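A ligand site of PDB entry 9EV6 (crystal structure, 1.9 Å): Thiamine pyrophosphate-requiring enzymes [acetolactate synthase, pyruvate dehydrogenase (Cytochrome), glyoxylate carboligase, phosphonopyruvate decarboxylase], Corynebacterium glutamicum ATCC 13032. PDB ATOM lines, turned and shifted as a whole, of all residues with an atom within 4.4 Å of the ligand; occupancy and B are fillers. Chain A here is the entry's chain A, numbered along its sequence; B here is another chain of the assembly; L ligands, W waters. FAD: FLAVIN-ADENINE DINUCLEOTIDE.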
ATOM      1  N   GLY A 211      24.027 -24.544 -26.276  1.00  0.00           N
ATOM      2  CA  GLY A 211      24.375 -25.212 -25.030  1.00  0.00           C
ATOM      3  C   GLY A 211      24.568 -26.704 -25.254  1.00  0.00           C
ATOM      4  O   GLY A 211      24.724 -27.154 -26.388  1.00  0.00           O
ATOM      5  N   ALA A 212      24.558 -27.476 -24.168  1.00  0.00           N
ATOM      6  CA  ALA A 212      24.763 -28.931 -24.204  1.00  0.00           C
ATOM      7  C   ALA A 212      23.756 -29.651 -25.115  1.00  0.00           C
ATOM      8  O   ALA A 212      24.080 -30.730 -25.615  1.00  0.00           O
ATOM      9  CB  ALA A 212      24.691 -29.525 -22.789  1.00  0.00           C
ATOM     10  N   GLY A 213      22.586 -29.063 -25.341  1.00  0.00           N
ATOM     11  CA  GLY A 213      21.557 -29.643 -26.193  1.00  0.00           C
ATOM     12  C   GLY A 213      21.931 -29.767 -27.657  1.00  0.00           C
ATOM     13  O   GLY A 213      21.228 -30.457 -28.383  1.00  0.00           O
ATOM     14  N   ALA A 235      27.137 -21.483 -24.387  1.00  0.00           N
ATOM     15  CA  ALA A 235      27.135 -21.567 -22.941  1.00  0.00           C
ATOM     16  C   ALA A 235      28.221 -22.569 -22.574  1.00  0.00           C
ATOM     17  O   ALA A 235      28.635 -23.393 -23.414  1.00  0.00           O
ATOM     18  CB  ALA A 235      25.750 -22.043 -22.441  1.00  0.00           C
ATOM     19  N   LEU A 236      28.694 -22.540 -21.330  1.00  0.00           N
ATOM     20  CA  LEU A 236      29.745 -23.441 -20.899  1.00  0.00           C
ATOM     21  C   LEU A 236      29.465 -24.938 -21.208  1.00  0.00           C
ATOM     22  O   LEU A 236      30.375 -25.656 -21.628  1.00  0.00           O
ATOM     23  CB  LEU A 236      29.978 -23.238 -19.395  1.00  0.00           C
ATOM     24  CG  LEU A 236      31.131 -24.027 -18.761  1.00  0.00           C
ATOM     25  CD1 LEU A 236      32.451 -23.776 -19.504  1.00  0.00           C
ATOM     26  CD2 LEU A 236      31.267 -23.646 -17.278  1.00  0.00           C
ATOM     27  N   GLY A 237      28.222 -25.387 -21.016  1.00  0.00           N
ATOM     28  CA  GLY A 237      27.866 -26.784 -21.265  1.00  0.00           C
ATOM     29  C   GLY A 237      27.899 -27.208 -22.724  1.00  0.00           C
ATOM     30  O   GLY A 237      27.961 -28.409 -23.015  1.00  0.00           O
ATOM     31  N   GLY A 238      27.873 -26.247 -23.649  1.00  0.00           N
ATOM     32  CA  GLY A 238      27.973 -26.536 -25.080  1.00  0.00           C
ATOM     33  C   GLY A 238      29.349 -26.368 -25.692  1.00  0.00           C
ATOM     34  O   GLY A 238      29.599 -26.757 -26.850  1.00  0.00           O
ATOM     35  N   MET A 252      32.037 -16.998 -25.424  1.00  0.00           N
ATOM     36  CA  MET A 252      31.097 -17.221 -24.347  1.00  0.00           C
ATOM     37  C   MET A 252      30.604 -15.926 -23.720  1.00  0.00           C
ATOM     38  O   MET A 252      31.226 -14.876 -23.821  1.00  0.00           O
ATOM     39  CB  MET A 252      31.810 -18.022 -23.263  1.00  0.00           C
ATOM     40  CG  MET A 252      32.133 -19.421 -23.679  1.00  0.00           C
ATOM     41  SD  MET A 252      32.787 -20.423 -22.310  1.00  0.00           S
ATOM     42  CE  MET A 252      31.589 -20.156 -21.129  1.00  0.00           C
ATOM     43  N   SER A 253      29.483 -16.038 -23.034  1.00  0.00           N
ATOM     44  CA  SER A 253      28.849 -14.957 -22.311  1.00  0.00           C
ATOM     45  C   SER A 253      28.960 -15.219 -20.783  1.00  0.00           C
ATOM     46  O   SER A 253      29.516 -16.236 -20.361  1.00  0.00           O
ATOM     47  CB  SER A 253      27.399 -14.844 -22.767  1.00  0.00           C
ATOM     48  OG  SER A 253      26.834 -13.646 -22.267  1.00  0.00           O
ATOM     49  N   GLY A 254      28.484 -14.276 -19.978  1.00  0.00           N
ATOM     50  CA  GLY A 254      28.581 -14.394 -18.522  1.00  0.00           C
ATOM     51  C   GLY A 254      29.888 -13.831 -17.992  1.00  0.00           C
ATOM     52  O   GLY A 254      30.732 -13.351 -18.763  1.00  0.00           O
ATOM     53  N   LEU A 255      30.103 -13.935 -16.686  1.00  0.00           N
ATOM     54  CA  LEU A 255      31.290 -13.386 -16.038  1.00  0.00           C
ATOM     55  C   LEU A 255      32.595 -14.070 -16.481  1.00  0.00           C
ATOM     56  O   LEU A 255      33.609 -13.369 -16.573  1.00  0.00           O
ATOM     57  CB  LEU A 255      31.119 -13.415 -14.524  1.00  0.00           C
ATOM     58  CG  LEU A 255      30.086 -12.387 -14.006  1.00  0.00           C
ATOM     59  CD1 LEU A 255      29.872 -12.542 -12.495  1.00  0.00           C
ATOM     60  CD2 LEU A 255      30.520 -10.937 -14.323  1.00  0.00           C
ATOM     61  N   LEU A 256      32.574 -15.378 -16.787  1.00  0.00           N
ATOM     62  CA  LEU A 256      33.817 -15.998 -17.299  1.00  0.00           C
ATOM     63  C   LEU A 256      33.857 -16.032 -18.857  1.00  0.00           C
ATOM     64  O   LEU A 256      34.739 -16.658 -19.437  1.00  0.00           O
ATOM     65  CB  LEU A 256      34.105 -17.381 -16.697  1.00  0.00           C
ATOM     66  CG  LEU A 256      33.035 -18.444 -16.724  1.00  0.00           C
ATOM     67  CD1 LEU A 256      32.834 -18.978 -18.111  1.00  0.00           C
ATOM     68  CD2 LEU A 256      33.430 -19.599 -15.865  1.00  0.00           C
ATOM     69  N   GLY A 257      32.953 -15.288 -19.488  1.00  0.00           N
ATOM     70  CA  GLY A 257      32.885 -15.188 -20.930  1.00  0.00           C
ATOM     71  C   GLY A 257      34.004 -14.351 -21.504  1.00  0.00           C
ATOM     72  O   GLY A 257      34.800 -13.758 -20.765  1.00  0.00           O
ATOM     73  N   GLY A 275      19.305 -25.438 -27.423  1.00  0.00           N
ATOM     74  CA  GLY A 275      19.656 -26.405 -26.380  1.00  0.00           C
ATOM     75  C   GLY A 275      20.471 -25.835 -25.239  1.00  0.00           C
ATOM     76  O   GLY A 275      21.524 -26.397 -24.899  1.00  0.00           O
ATOM     77  N   THR A 276      19.999 -24.731 -24.632  1.00  0.00           N
ATOM     78  CA  THR A 276      20.753 -24.103 -23.546  1.00  0.00           C
ATOM     79  C   THR A 276      19.839 -23.625 -22.448  1.00  0.00           C
ATOM     80  O   THR A 276      18.712 -23.207 -22.694  1.00  0.00           O
ATOM     81  CB  THR A 276      21.626 -22.924 -24.071  1.00  0.00           C
ATOM     82  OG1 THR A 276      22.300 -22.299 -22.974  1.00  0.00           O
ATOM     83  CG2 THR A 276      20.819 -21.875 -24.814  1.00  0.00           C
ATOM     84  N   ASP A 277      20.332 -23.681 -21.229  1.00  0.00           N
ATOM     85  CA  ASP A 277      19.598 -23.174 -20.081  1.00  0.00           C
ATOM     86  C   ASP A 277      20.505 -22.195 -19.294  1.00  0.00           C
ATOM     87  O   ASP A 277      20.405 -22.113 -18.077  1.00  0.00           O
ATOM     88  CB  ASP A 277      19.047 -24.315 -19.206  1.00  0.00           C
ATOM     89  CG  ASP A 277      18.022 -23.868 -18.178  1.00  0.00           C
ATOM     90  OD1 ASP A 277      17.232 -22.918 -18.469  1.00  0.00           O
ATOM     91  OD2 ASP A 277      18.036 -24.415 -17.059  1.00  0.00           O
ATOM     92  N   PHE A 278      21.381 -21.430 -20.012  1.00  0.00           N
ATOM     93  CA  PHE A 278      22.294 -20.413 -19.496  1.00  0.00           C
ATOM     94  C   PHE A 278      21.546 -19.492 -18.560  1.00  0.00           C
ATOM     95  O   PHE A 278      20.580 -18.881 -18.983  1.00  0.00           O
ATOM     96  CB  PHE A 278      22.841 -19.622 -20.683  1.00  0.00           C
ATOM     97  CG  PHE A 278      23.720 -18.441 -20.362  1.00  0.00           C
ATOM     98  CD1 PHE A 278      25.084 -18.598 -20.211  1.00  0.00           C
ATOM     99  CD2 PHE A 278      23.194 -17.158 -20.349  1.00  0.00           C
ATOM    100  CE1 PHE A 278      25.914 -17.495 -19.995  1.00  0.00           C
ATOM    101  CE2 PHE A 278      24.025 -16.052 -20.123  1.00  0.00           C
ATOM    102  CZ  PHE A 278      25.370 -16.229 -19.941  1.00  0.00           C
ATOM    103  N   PRO A 279      21.901 -19.483 -17.271  1.00  0.00           N
ATOM    104  CA  PRO A 279      21.023 -18.815 -16.290  1.00  0.00           C
ATOM    105  C   PRO A 279      21.215 -17.328 -16.051  1.00  0.00           C
ATOM    106  O   PRO A 279      20.404 -16.739 -15.329  1.00  0.00           O
ATOM    107  CB  PRO A 279      21.339 -19.558 -14.991  1.00  0.00           C
ATOM    108  CG  PRO A 279      22.736 -20.002 -15.148  1.00  0.00           C
ATOM    109  CD  PRO A 279      22.933 -20.298 -16.611  1.00  0.00           C
ATOM    110  N   TYR A 280      22.254 -16.715 -16.607  1.00  0.00           N
ATOM    111  CA  TYR A 280      22.566 -15.306 -16.303  1.00  0.00           C
ATOM    112  C   TYR A 280      21.786 -14.337 -17.203  1.00  0.00           C
ATOM    113  O   TYR A 280      22.326 -13.779 -18.154  1.00  0.00           O
ATOM    114  CB  TYR A 280      24.085 -15.065 -16.382  1.00  0.00           C
ATOM    115  CG  TYR A 280      24.831 -16.144 -15.609  1.00  0.00           C
ATOM    116  CD1 TYR A 280      24.689 -16.256 -14.230  1.00  0.00           C
ATOM    117  CD2 TYR A 280      25.529 -17.143 -16.274  1.00  0.00           C
ATOM    118  CE1 TYR A 280      25.313 -17.278 -13.526  1.00  0.00           C
ATOM    119  CE2 TYR A 280      26.150 -18.182 -15.585  1.00  0.00           C
ATOM    120  CZ  TYR A 280      26.021 -18.254 -14.211  1.00  0.00           C
ATOM    121  OH  TYR A 280      26.581 -19.299 -13.522  1.00  0.00           O
ATOM    122  N   VAL A 292      14.907 -23.202 -28.721  1.00  0.00           N
ATOM    123  CA  VAL A 292      14.605 -24.594 -29.034  1.00  0.00           C
ATOM    124  C   VAL A 292      15.079 -25.441 -27.879  1.00  0.00           C
ATOM    125  O   VAL A 292      16.274 -25.422 -27.565  1.00  0.00           O
ATOM    126  CB  VAL A 292      15.258 -25.039 -30.344  1.00  0.00           C
ATOM    127  CG1 VAL A 292      14.912 -26.496 -30.637  1.00  0.00           C
ATOM    128  CG2 VAL A 292      14.830 -24.123 -31.508  1.00  0.00           C
ATOM    129  N   ASP A 293      14.162 -26.169 -27.211  1.00  0.00           N
ATOM    130  CA  ASP A 293      14.558 -27.040 -26.102  1.00  0.00           C
ATOM    131  C   ASP A 293      13.721 -28.311 -26.139  1.00  0.00           C
ATOM    132  O   ASP A 293      12.539 -28.246 -26.399  1.00  0.00           O
ATOM    133  CB  ASP A 293      14.388 -26.346 -24.743  1.00  0.00           C
ATOM    134  CG  ASP A 293      15.329 -26.937 -23.692  1.00  0.00           C
ATOM    135  OD1 ASP A 293      15.060 -28.072 -23.222  1.00  0.00           O
ATOM    136  OD2 ASP A 293      16.351 -26.276 -23.373  1.00  0.00           O
ATOM    137  N   ILE A 294      14.343 -29.451 -25.841  1.00  0.00           N
ATOM    138  CA  ILE A 294      13.677 -30.752 -25.847  1.00  0.00           C
ATOM    139  C   ILE A 294      12.694 -30.876 -24.683  1.00  0.00           C
ATOM    140  O   ILE A 294      11.767 -31.663 -24.754  1.00  0.00           O
ATOM    141  CB  ILE A 294      14.730 -31.904 -25.862  1.00  0.00           C
ATOM    142  CG1 ILE A 294      14.136 -33.202 -26.458  1.00  0.00           C
ATOM    143  CG2 ILE A 294      15.364 -32.141 -24.478  1.00  0.00           C
ATOM    144  CD1 ILE A 294      15.133 -34.197 -26.865  1.00  0.00           C
ATOM    145  N   ASN A 295      12.906 -30.111 -23.595  1.00  0.00           N
ATOM    146  CA  ASN A 295      12.023 -30.112 -22.456  1.00  0.00           C
ATOM    147  C   ASN A 295      11.265 -28.778 -22.483  1.00  0.00           C
ATOM    148  O   ASN A 295      11.837 -27.735 -22.178  1.00  0.00           O
ATOM    149  CB  ASN A 295      12.815 -30.318 -21.137  1.00  0.00           C
ATOM    150  CG  ASN A 295      11.897 -30.449 -19.925  1.00  0.00           C
ATOM    151  OD1 ASN A 295      10.749 -29.982 -19.928  1.00  0.00           O
ATOM    152  ND2 ASN A 295      12.360 -31.095 -18.863  1.00  0.00           N
ATOM    153  N   HIS A 298      11.496 -25.953 -19.808  1.00  0.00           N
ATOM    154  CA  HIS A 298      12.695 -25.112 -19.696  1.00  0.00           C
ATOM    155  C   HIS A 298      12.612 -23.857 -20.558  1.00  0.00           C
ATOM    156  O   HIS A 298      13.484 -22.995 -20.410  1.00  0.00           O
ATOM    157  CB  HIS A 298      13.954 -25.883 -20.123  1.00  0.00           C
ATOM    158  CG  HIS A 298      14.318 -27.054 -19.254  1.00  0.00           C
ATOM    159  ND1 HIS A 298      15.519 -27.739 -19.426  1.00  0.00           N
ATOM    160  CD2 HIS A 298      13.630 -27.639 -18.252  1.00  0.00           C
ATOM    161  CE1 HIS A 298      15.501 -28.710 -18.535  1.00  0.00           C
ATOM    162  NE2 HIS A 298      14.383 -28.704 -17.818  1.00  0.00           N
ATOM    163  N   GLY A 311      11.424 -29.154 -28.985  1.00  0.00           N
ATOM    164  CA  GLY A 311      11.966 -30.096 -29.950  1.00  0.00           C
ATOM    165  C   GLY A 311      13.465 -30.272 -29.832  1.00  0.00           C
ATOM    166  O   GLY A 311      14.142 -29.514 -29.126  1.00  0.00           O
ATOM    167  N   ASP A 312      13.961 -31.298 -30.481  1.00  0.00           N
ATOM    168  CA  ASP A 312      15.369 -31.618 -30.535  1.00  0.00           C
ATOM    169  C   ASP A 312      16.053 -30.612 -31.465  1.00  0.00           C
ATOM    170  O   ASP A 312      15.450 -30.228 -32.477  1.00  0.00           O
ATOM    171  CB  ASP A 312      15.496 -33.043 -31.075  1.00  0.00           C
ATOM    172  CG  ASP A 312      16.894 -33.495 -31.401  1.00  0.00           C
ATOM    173  OD1 ASP A 312      17.660 -33.804 -30.449  1.00  0.00           O
ATOM    174  OD2 ASP A 312      17.227 -33.570 -32.620  1.00  0.00           O
ATOM    175  N   VAL A 313      17.268 -30.165 -31.148  1.00  0.00           N
ATOM    176  CA  VAL A 313      17.957 -29.185 -32.004  1.00  0.00           C
ATOM    177  C   VAL A 313      18.175 -29.727 -33.435  1.00  0.00           C
ATOM    178  O   VAL A 313      17.774 -29.067 -34.393  1.00  0.00           O
ATOM    179  CB  VAL A 313      19.277 -28.687 -31.388  1.00  0.00           C
ATOM    180  CG1 VAL A 313      20.043 -27.808 -32.390  1.00  0.00           C
ATOM    181  CG2 VAL A 313      19.026 -27.925 -30.087  1.00  0.00           C
ATOM    182  N   THR A 384      35.157 -26.508  -9.324  1.00  0.00           N
ATOM    183  CA  THR A 384      34.406 -25.256  -9.312  1.00  0.00           C
ATOM    184  C   THR A 384      35.229 -24.123  -8.698  1.00  0.00           C
ATOM    185  O   THR A 384      35.779 -24.278  -7.623  1.00  0.00           O
ATOM    186  CB  THR A 384      33.102 -25.451  -8.560  1.00  0.00           C
ATOM    187  OG1 THR A 384      32.364 -26.448  -9.257  1.00  0.00           O
ATOM    188  CG2 THR A 384      32.298 -24.164  -8.403  1.00  0.00           C
ATOM    189  N   GLY A 385      35.302 -23.006  -9.392  1.00  0.00           N
ATOM    190  CA  GLY A 385      36.080 -21.847  -8.942  1.00  0.00           C
ATOM    191  C   GLY A 385      36.806 -21.226 -10.102  1.00  0.00           C
ATOM    192  O   GLY A 385      36.302 -21.278 -11.238  1.00  0.00           O
ATOM    193  N   ASN A 388      37.249 -22.939 -13.509  1.00  0.00           N
ATOM    194  CA  ASN A 388      36.222 -22.836 -14.565  1.00  0.00           C
ATOM    195  C   ASN A 388      36.593 -21.763 -15.562  1.00  0.00           C
ATOM    196  O   ASN A 388      36.318 -21.915 -16.735  1.00  0.00           O
ATOM    197  CB  ASN A 388      34.819 -22.575 -14.008  1.00  0.00           C
ATOM    198  CG  ASN A 388      34.263 -23.742 -13.263  1.00  0.00           C
ATOM    199  OD1 ASN A 388      34.121 -23.703 -12.024  1.00  0.00           O
ATOM    200  ND2 ASN A 388      33.951 -24.819 -13.967  1.00  0.00           N
ATOM    201  N   SER A 407      31.231 -29.466 -12.384  1.00  0.00           N
ATOM    202  CA  SER A 407      30.000 -29.164 -11.661  1.00  0.00           C
ATOM    203  C   SER A 407      29.446 -27.854 -12.244  1.00  0.00           C
ATOM    204  O   SER A 407      29.327 -26.851 -11.541  1.00  0.00           O
ATOM    205  CB  SER A 407      30.273 -29.064 -10.169  1.00  0.00           C
ATOM    206  OG  SER A 407      29.026 -29.009  -9.483  1.00  0.00           O
ATOM    207  N   PHE A 408      29.151 -27.860 -13.542  1.00  0.00           N
ATOM    208  CA  PHE A 408      28.737 -26.653 -14.235  1.00  0.00           C
ATOM    209  C   PHE A 408      27.384 -26.128 -13.824  1.00  0.00           C
ATOM    210  O   PHE A 408      27.152 -24.935 -14.010  1.00  0.00           O
ATOM    211  CB  PHE A 408      28.764 -26.856 -15.763  1.00  0.00           C
ATOM    212  CG  PHE A 408      30.110 -27.312 -16.305  1.00  0.00           C
ATOM    213  CD1 PHE A 408      31.291 -26.823 -15.763  1.00  0.00           C
ATOM    214  CD2 PHE A 408      30.194 -28.237 -17.321  1.00  0.00           C
ATOM    215  CE1 PHE A 408      32.534 -27.252 -16.248  1.00  0.00           C
ATOM    216  CE2 PHE A 408      31.427 -28.650 -17.822  1.00  0.00           C
ATOM    217  CZ  PHE A 408      32.588 -28.165 -17.265  1.00  0.00           C
ATOM    218  N   ARG A 409      26.479 -26.980 -13.317  1.00  0.00           N
ATOM    219  CA  ARG A 409      25.133 -26.516 -12.981  1.00  0.00           C
ATOM    220  C   ARG A 409      24.910 -26.447 -11.474  1.00  0.00           C
ATOM    221  O   ARG A 409      24.408 -25.442 -10.966  1.00  0.00           O
ATOM    222  CB  ARG A 409      24.095 -27.384 -13.662  1.00  0.00           C
ATOM    223  CG  ARG A 409      24.303 -27.391 -15.178  1.00  0.00           C
ATOM    224  CD  ARG A 409      24.277 -28.781 -15.764  1.00  0.00           C
ATOM    225  NE  ARG A 409      24.401 -28.772 -17.221  1.00  0.00           N
ATOM    226  CZ  ARG A 409      25.399 -29.353 -17.896  1.00  0.00           C
ATOM    227  NH1 ARG A 409      26.343 -30.018 -17.247  1.00  0.00           N
ATOM    228  NH2 ARG A 409      25.431 -29.290 -19.221  1.00  0.00           N
ATOM    229  N   GLY A 411      27.366 -26.391  -9.318  1.00  0.00           N
ATOM    230  CA  GLY A 411      28.422 -25.504  -8.872  1.00  0.00           C
ATOM    231  C   GLY A 411      29.052 -25.845  -7.536  1.00  0.00           C
ATOM    232  O   GLY A 411      29.318 -24.936  -6.743  1.00  0.00           O
ATOM    233  N   MET A 470      37.919 -17.490  -6.536  1.00  0.00           N
ATOM    234  CA  MET A 470      36.662 -17.023  -7.104  1.00  0.00           C
ATOM    235  C   MET A 470      35.952 -16.075  -6.118  1.00  0.00           C
ATOM    236  O   MET A 470      35.375 -15.069  -6.544  1.00  0.00           O
ATOM    237  CB  MET A 470      35.816 -18.244  -7.468  1.00  0.00           C
ATOM    238  CG  MET A 470      34.368 -17.948  -7.776  1.00  0.00           C
ATOM    239  SD  MET A 470      34.109 -17.218  -9.389  1.00  0.00           S
ATOM    240  CE  MET A 470      34.591 -18.512 -10.422  1.00  0.00           C
ATOM    241  N   PHE B 113      21.701 -21.595 -11.094  1.00  0.00           N
ATOM    242  CA  PHE B 113      23.008 -22.122 -10.769  1.00  0.00           C
ATOM    243  C   PHE B 113      23.125 -22.331  -9.240  1.00  0.00           C
ATOM    244  O   PHE B 113      22.752 -21.427  -8.467  1.00  0.00           O
ATOM    245  CB  PHE B 113      24.043 -21.087 -11.253  1.00  0.00           C
ATOM    246  CG  PHE B 113      25.474 -21.355 -10.846  1.00  0.00           C
ATOM    247  CD1 PHE B 113      26.131 -22.502 -11.280  1.00  0.00           C
ATOM    248  CD2 PHE B 113      26.172 -20.444 -10.070  1.00  0.00           C
ATOM    249  CE1 PHE B 113      27.448 -22.725 -10.938  1.00  0.00           C
ATOM    250  CE2 PHE B 113      27.489 -20.688  -9.699  1.00  0.00           C
ATOM    251  CZ  PHE B 113      28.125 -21.806 -10.173  1.00  0.00           C
HETATM  252  PA  FAD L   1      22.303 -26.919 -19.475  1.00  0.00           P
HETATM  253  O1A FAD L   1      22.036 -25.833 -18.514  1.00  0.00           O
HETATM  254  O2A FAD L   1      22.389 -28.303 -18.963  1.00  0.00           O
HETATM  255  O5B FAD L   1      21.189 -26.795 -20.602  1.00  0.00           O
HETATM  256  C5B FAD L   1      21.093 -27.760 -21.665  1.00  0.00           C
HETATM  257  C4B FAD L   1      19.700 -27.588 -22.214  1.00  0.00           C
HETATM  258  O4B FAD L   1      19.566 -28.312 -23.467  1.00  0.00           O
HETATM  259  C3B FAD L   1      18.569 -28.063 -21.299  1.00  0.00           C
HETATM  260  O3B FAD L   1      17.526 -27.098 -21.207  1.00  0.00           O
HETATM  261  C2B FAD L   1      18.108 -29.364 -21.965  1.00  0.00           C
HETATM  262  O2B FAD L   1      16.726 -29.593 -21.749  1.00  0.00           O
HETATM  263  C1B FAD L   1      18.351 -29.035 -23.437  1.00  0.00           C
HETATM  264  N9A FAD L   1      18.479 -30.179 -24.315  1.00  0.00           N
HETATM  265  C8A FAD L   1      19.142 -31.354 -24.075  1.00  0.00           C
HETATM  266  N7A FAD L   1      19.184 -32.174 -25.102  1.00  0.00           N
HETATM  267  C5A FAD L   1      18.500 -31.490 -26.094  1.00  0.00           C
HETATM  268  C6A FAD L   1      18.264 -31.776 -27.449  1.00  0.00           C
HETATM  269  N6A FAD L   1      18.664 -32.906 -28.048  1.00  0.00           N
HETATM  270  N1A FAD L   1      17.630 -30.830 -28.189  1.00  0.00           N
HETATM  271  C2A FAD L   1      17.260 -29.694 -27.597  1.00  0.00           C
HETATM  272  N3A FAD L   1      17.424 -29.319 -26.329  1.00  0.00           N
HETATM  273  C4A FAD L   1      18.056 -30.256 -25.624  1.00  0.00           C
HETATM  274  N1  FAD L   1      28.452 -20.607 -17.934  1.00  0.00           N
HETATM  275  C2  FAD L   1      28.630 -19.625 -18.861  1.00  0.00           C
HETATM  276  O2  FAD L   1      28.388 -19.823 -20.065  1.00  0.00           O
HETATM  277  N3  FAD L   1      29.175 -18.418 -18.462  1.00  0.00           N
HETATM  278  C4  FAD L   1      29.579 -18.092 -17.176  1.00  0.00           C
HETATM  279  O4  FAD L   1      30.030 -16.971 -16.936  1.00  0.00           O
HETATM  280  C4X FAD L   1      29.419 -19.147 -16.214  1.00  0.00           C
HETATM  281  N5  FAD L   1      29.985 -19.002 -15.046  1.00  0.00           N
HETATM  282  C5X FAD L   1      30.042 -20.099 -14.194  1.00  0.00           C
HETATM  283  C6  FAD L   1      30.842 -20.011 -13.059  1.00  0.00           C
HETATM  284  C7  FAD L   1      31.111 -21.136 -12.280  1.00  0.00           C
HETATM  285  C7M FAD L   1      31.967 -21.001 -11.040  1.00  0.00           C
HETATM  286  C8  FAD L   1      30.542 -22.397 -12.656  1.00  0.00           C
HETATM  287  C8M FAD L   1      30.801 -23.645 -11.864  1.00  0.00           C
HETATM  288  C9  FAD L   1      29.734 -22.472 -13.785  1.00  0.00           C
HETATM  289  C9A FAD L   1      29.478 -21.341 -14.546  1.00  0.00           C
HETATM  290  N10 FAD L   1      28.789 -21.427 -15.773  1.00  0.00           N
HETATM  291  C10 FAD L   1      28.824 -20.375 -16.675  1.00  0.00           C
HETATM  292  C1' FAD L   1      27.835 -22.523 -16.018  1.00  0.00           C
HETATM  293  C2' FAD L   1      26.390 -22.029 -15.991  1.00  0.00           C
HETATM  294  O2' FAD L   1      25.962 -21.799 -14.654  1.00  0.00           O
HETATM  295  C3' FAD L   1      25.469 -23.054 -16.674  1.00  0.00           C
HETATM  296  O3' FAD L   1      25.562 -24.316 -16.003  1.00  0.00           O
HETATM  297  C4' FAD L   1      25.759 -23.298 -18.158  1.00  0.00           C
HETATM  298  O4' FAD L   1      26.085 -22.089 -18.823  1.00  0.00           O
HETATM  299  C5' FAD L   1      24.622 -24.040 -18.829  1.00  0.00           C
HETATM  300  O5' FAD L   1      25.170 -24.709 -19.979  1.00  0.00           O
HETATM  301  P   FAD L   1      24.204 -25.319 -21.075  1.00  0.00           P
HETATM  302  O1P FAD L   1      25.043 -25.853 -22.164  1.00  0.00           O
HETATM  303  O2P FAD L   1      23.132 -24.348 -21.378  1.00  0.00           O
HETATM  304  O3P FAD L   1      23.645 -26.592 -20.269  1.00  0.00           O
HETATM  305  O   HOH W   1      19.032 -35.903 -29.745  1.00  0.00           O
HETATM  306  O   HOH W   2      23.215 -23.599 -14.036  1.00  0.00           O
HETATM  307  O   HOH W   3      29.782 -16.457 -13.507  1.00  0.00           O
HETATM  308  O   HOH W   4      21.127 -30.995 -19.006  1.00  0.00           O
HETATM  309  O   HOH W   5      21.185 -34.842 -27.805  1.00  0.00           O
HETATM  310  O   HOH W   6      21.634 -32.790 -29.319  1.00  0.00           O
HETATM  311  O   HOH W   7      21.797 -23.894 -16.482  1.00  0.00           O
HETATM  312  O   HOH W   8      27.994 -15.167 -14.784  1.00  0.00           O
HETATM  313  O   HOH W   9      28.320 -18.401 -22.405  1.00  0.00           O
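The backbone carbonyl oxygen of Gly 275 sits close to an oxygen (O4B) of the ligand (3.1 Å). Merely in contact with the ligand: Gly 211, Gly 213, Ala 235, Met 252, Gly 254, Phe 278, Pro 279, Gly 311, Thr 384, Asn 388, Ser 407, Met 470 and Phe 113 of chain B.
The side-chain amide oxygen of Asn 388 sits at hydrogen-bond distance from the backbone NH of Gly 385, at 3.0 Å. The backbone carbonyl oxygen (O) of Gly 275 lies within hydrogen-bond range of the backbone NH (N) of Ala 212, 3.3 Å away. The backbone carbonyl oxygen (O) of Gly 311 lies within hydrogen-bond range of the backbone NH (N) of Ile 294 (3.3 Å). The backbone carbonyl oxygen of Gly 275 lies within hydrogen-bond range of the backbone NH of Gly 213 (2.9 Å). The backbone carbonyl oxygen of Val 292 sits at hydrogen-bond distance from the backbone NH of Gly 275 (3.0 Å). The side-chain hydroxyl (OG1) of Thr 276 is in hydrogen-bond range of the backbone NH (N) of Phe 278 (3.2 Å). The backbone NH (N) of Gly 411 lies within hydrogen-bond range of the side-chain hydroxyl (OG) of Ser 407 (3.1 Å). The side-chain carboxylate (OD1) of Asp 293 is in hydrogen-bond range of the backbone NH (N) of Asn 295 (3.0 Å).
An oxygen (O2P) of the ligand is in hydrogen-bond range of the backbone NH (N) of Asp 277, at 2.9 Å. A nitrogen (N3A) of the ligand is in hydrogen-bond range of the backbone NH (N) of Ile 294, at 3.1 Å. A nitrogen (N6A) of the ligand sits at hydrogen-bond distance from the side-chain carboxylate of Asp 312 (2.8 Å). N of Val 313 lies within hydrogen-bond range of N1A of the ligand (3.1 Å). O2P of the ligand is in hydrogen-bond range of OG1 of Thr 276. The backbone NH (N) of Gly 237 sits at hydrogen-bond distance from an oxygen (O5') of the ligand. OH of Tyr 280 sits at hydrogen-bond distance from O2' of the ligand (2.8 Å). N of Ala 212 lies within hydrogen-bond range of O1P of the ligand (2.6 Å). The backbone NH (N) of Leu 255 is in hydrogen-bond range of an oxygen (O4) of the ligand (3.0 Å). NE of Arg 409 lies within salt-bridge range of O2A of the ligand. O3B of the ligand sits at hydrogen-bond distance from ND1 of His 298 (2.8 Å). N of Gly 238 sits at hydrogen-bond distance from O1P of the ligand (3.2 Å). N of Leu 236 lies within hydrogen-bond range of O2 of the ligand (3.0 Å). The side-chain carboxylate (OD2) of Asp 293 is in hydrogen-bond range of an oxygen (O3B) of the ligand. N of Leu 256 is in hydrogen-bond range of O4 of the ligand, 3.0 Å away. The backbone carbonyl oxygen (O) of Phe 408 is in hydrogen-bond range of an oxygen (O3') of the ligand, at 2.6 Å. The backbone carbonyl oxygen (O) of Ser 253 sits at hydrogen-bond distance from a nitrogen (N3) of the ligand (2.9 Å).
Water W9 bridges the backbone NH of Ser 253 (2.7 Å) and an oxygen (O2) of the ligand (2.7 Å). Water W7 lies within hydrogen-bond range of the backbone carbonyl oxygen (O) of Asp 277 and an oxygen (O1A) of the ligand. Water W6 bridges the backbone carbonyl oxygen of Gly 213 (2.5 Å) and a nitrogen (N6A) of the ligand (3.2 Å). Water W1 lies within hydrogen-bond range of the side-chain carboxylate of Asp 312 (2.6 Å) and a nitrogen (N6A) of the ligand (3.5 Å). Water W8 bridges N of Leu 255 and O4 of the ligand.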
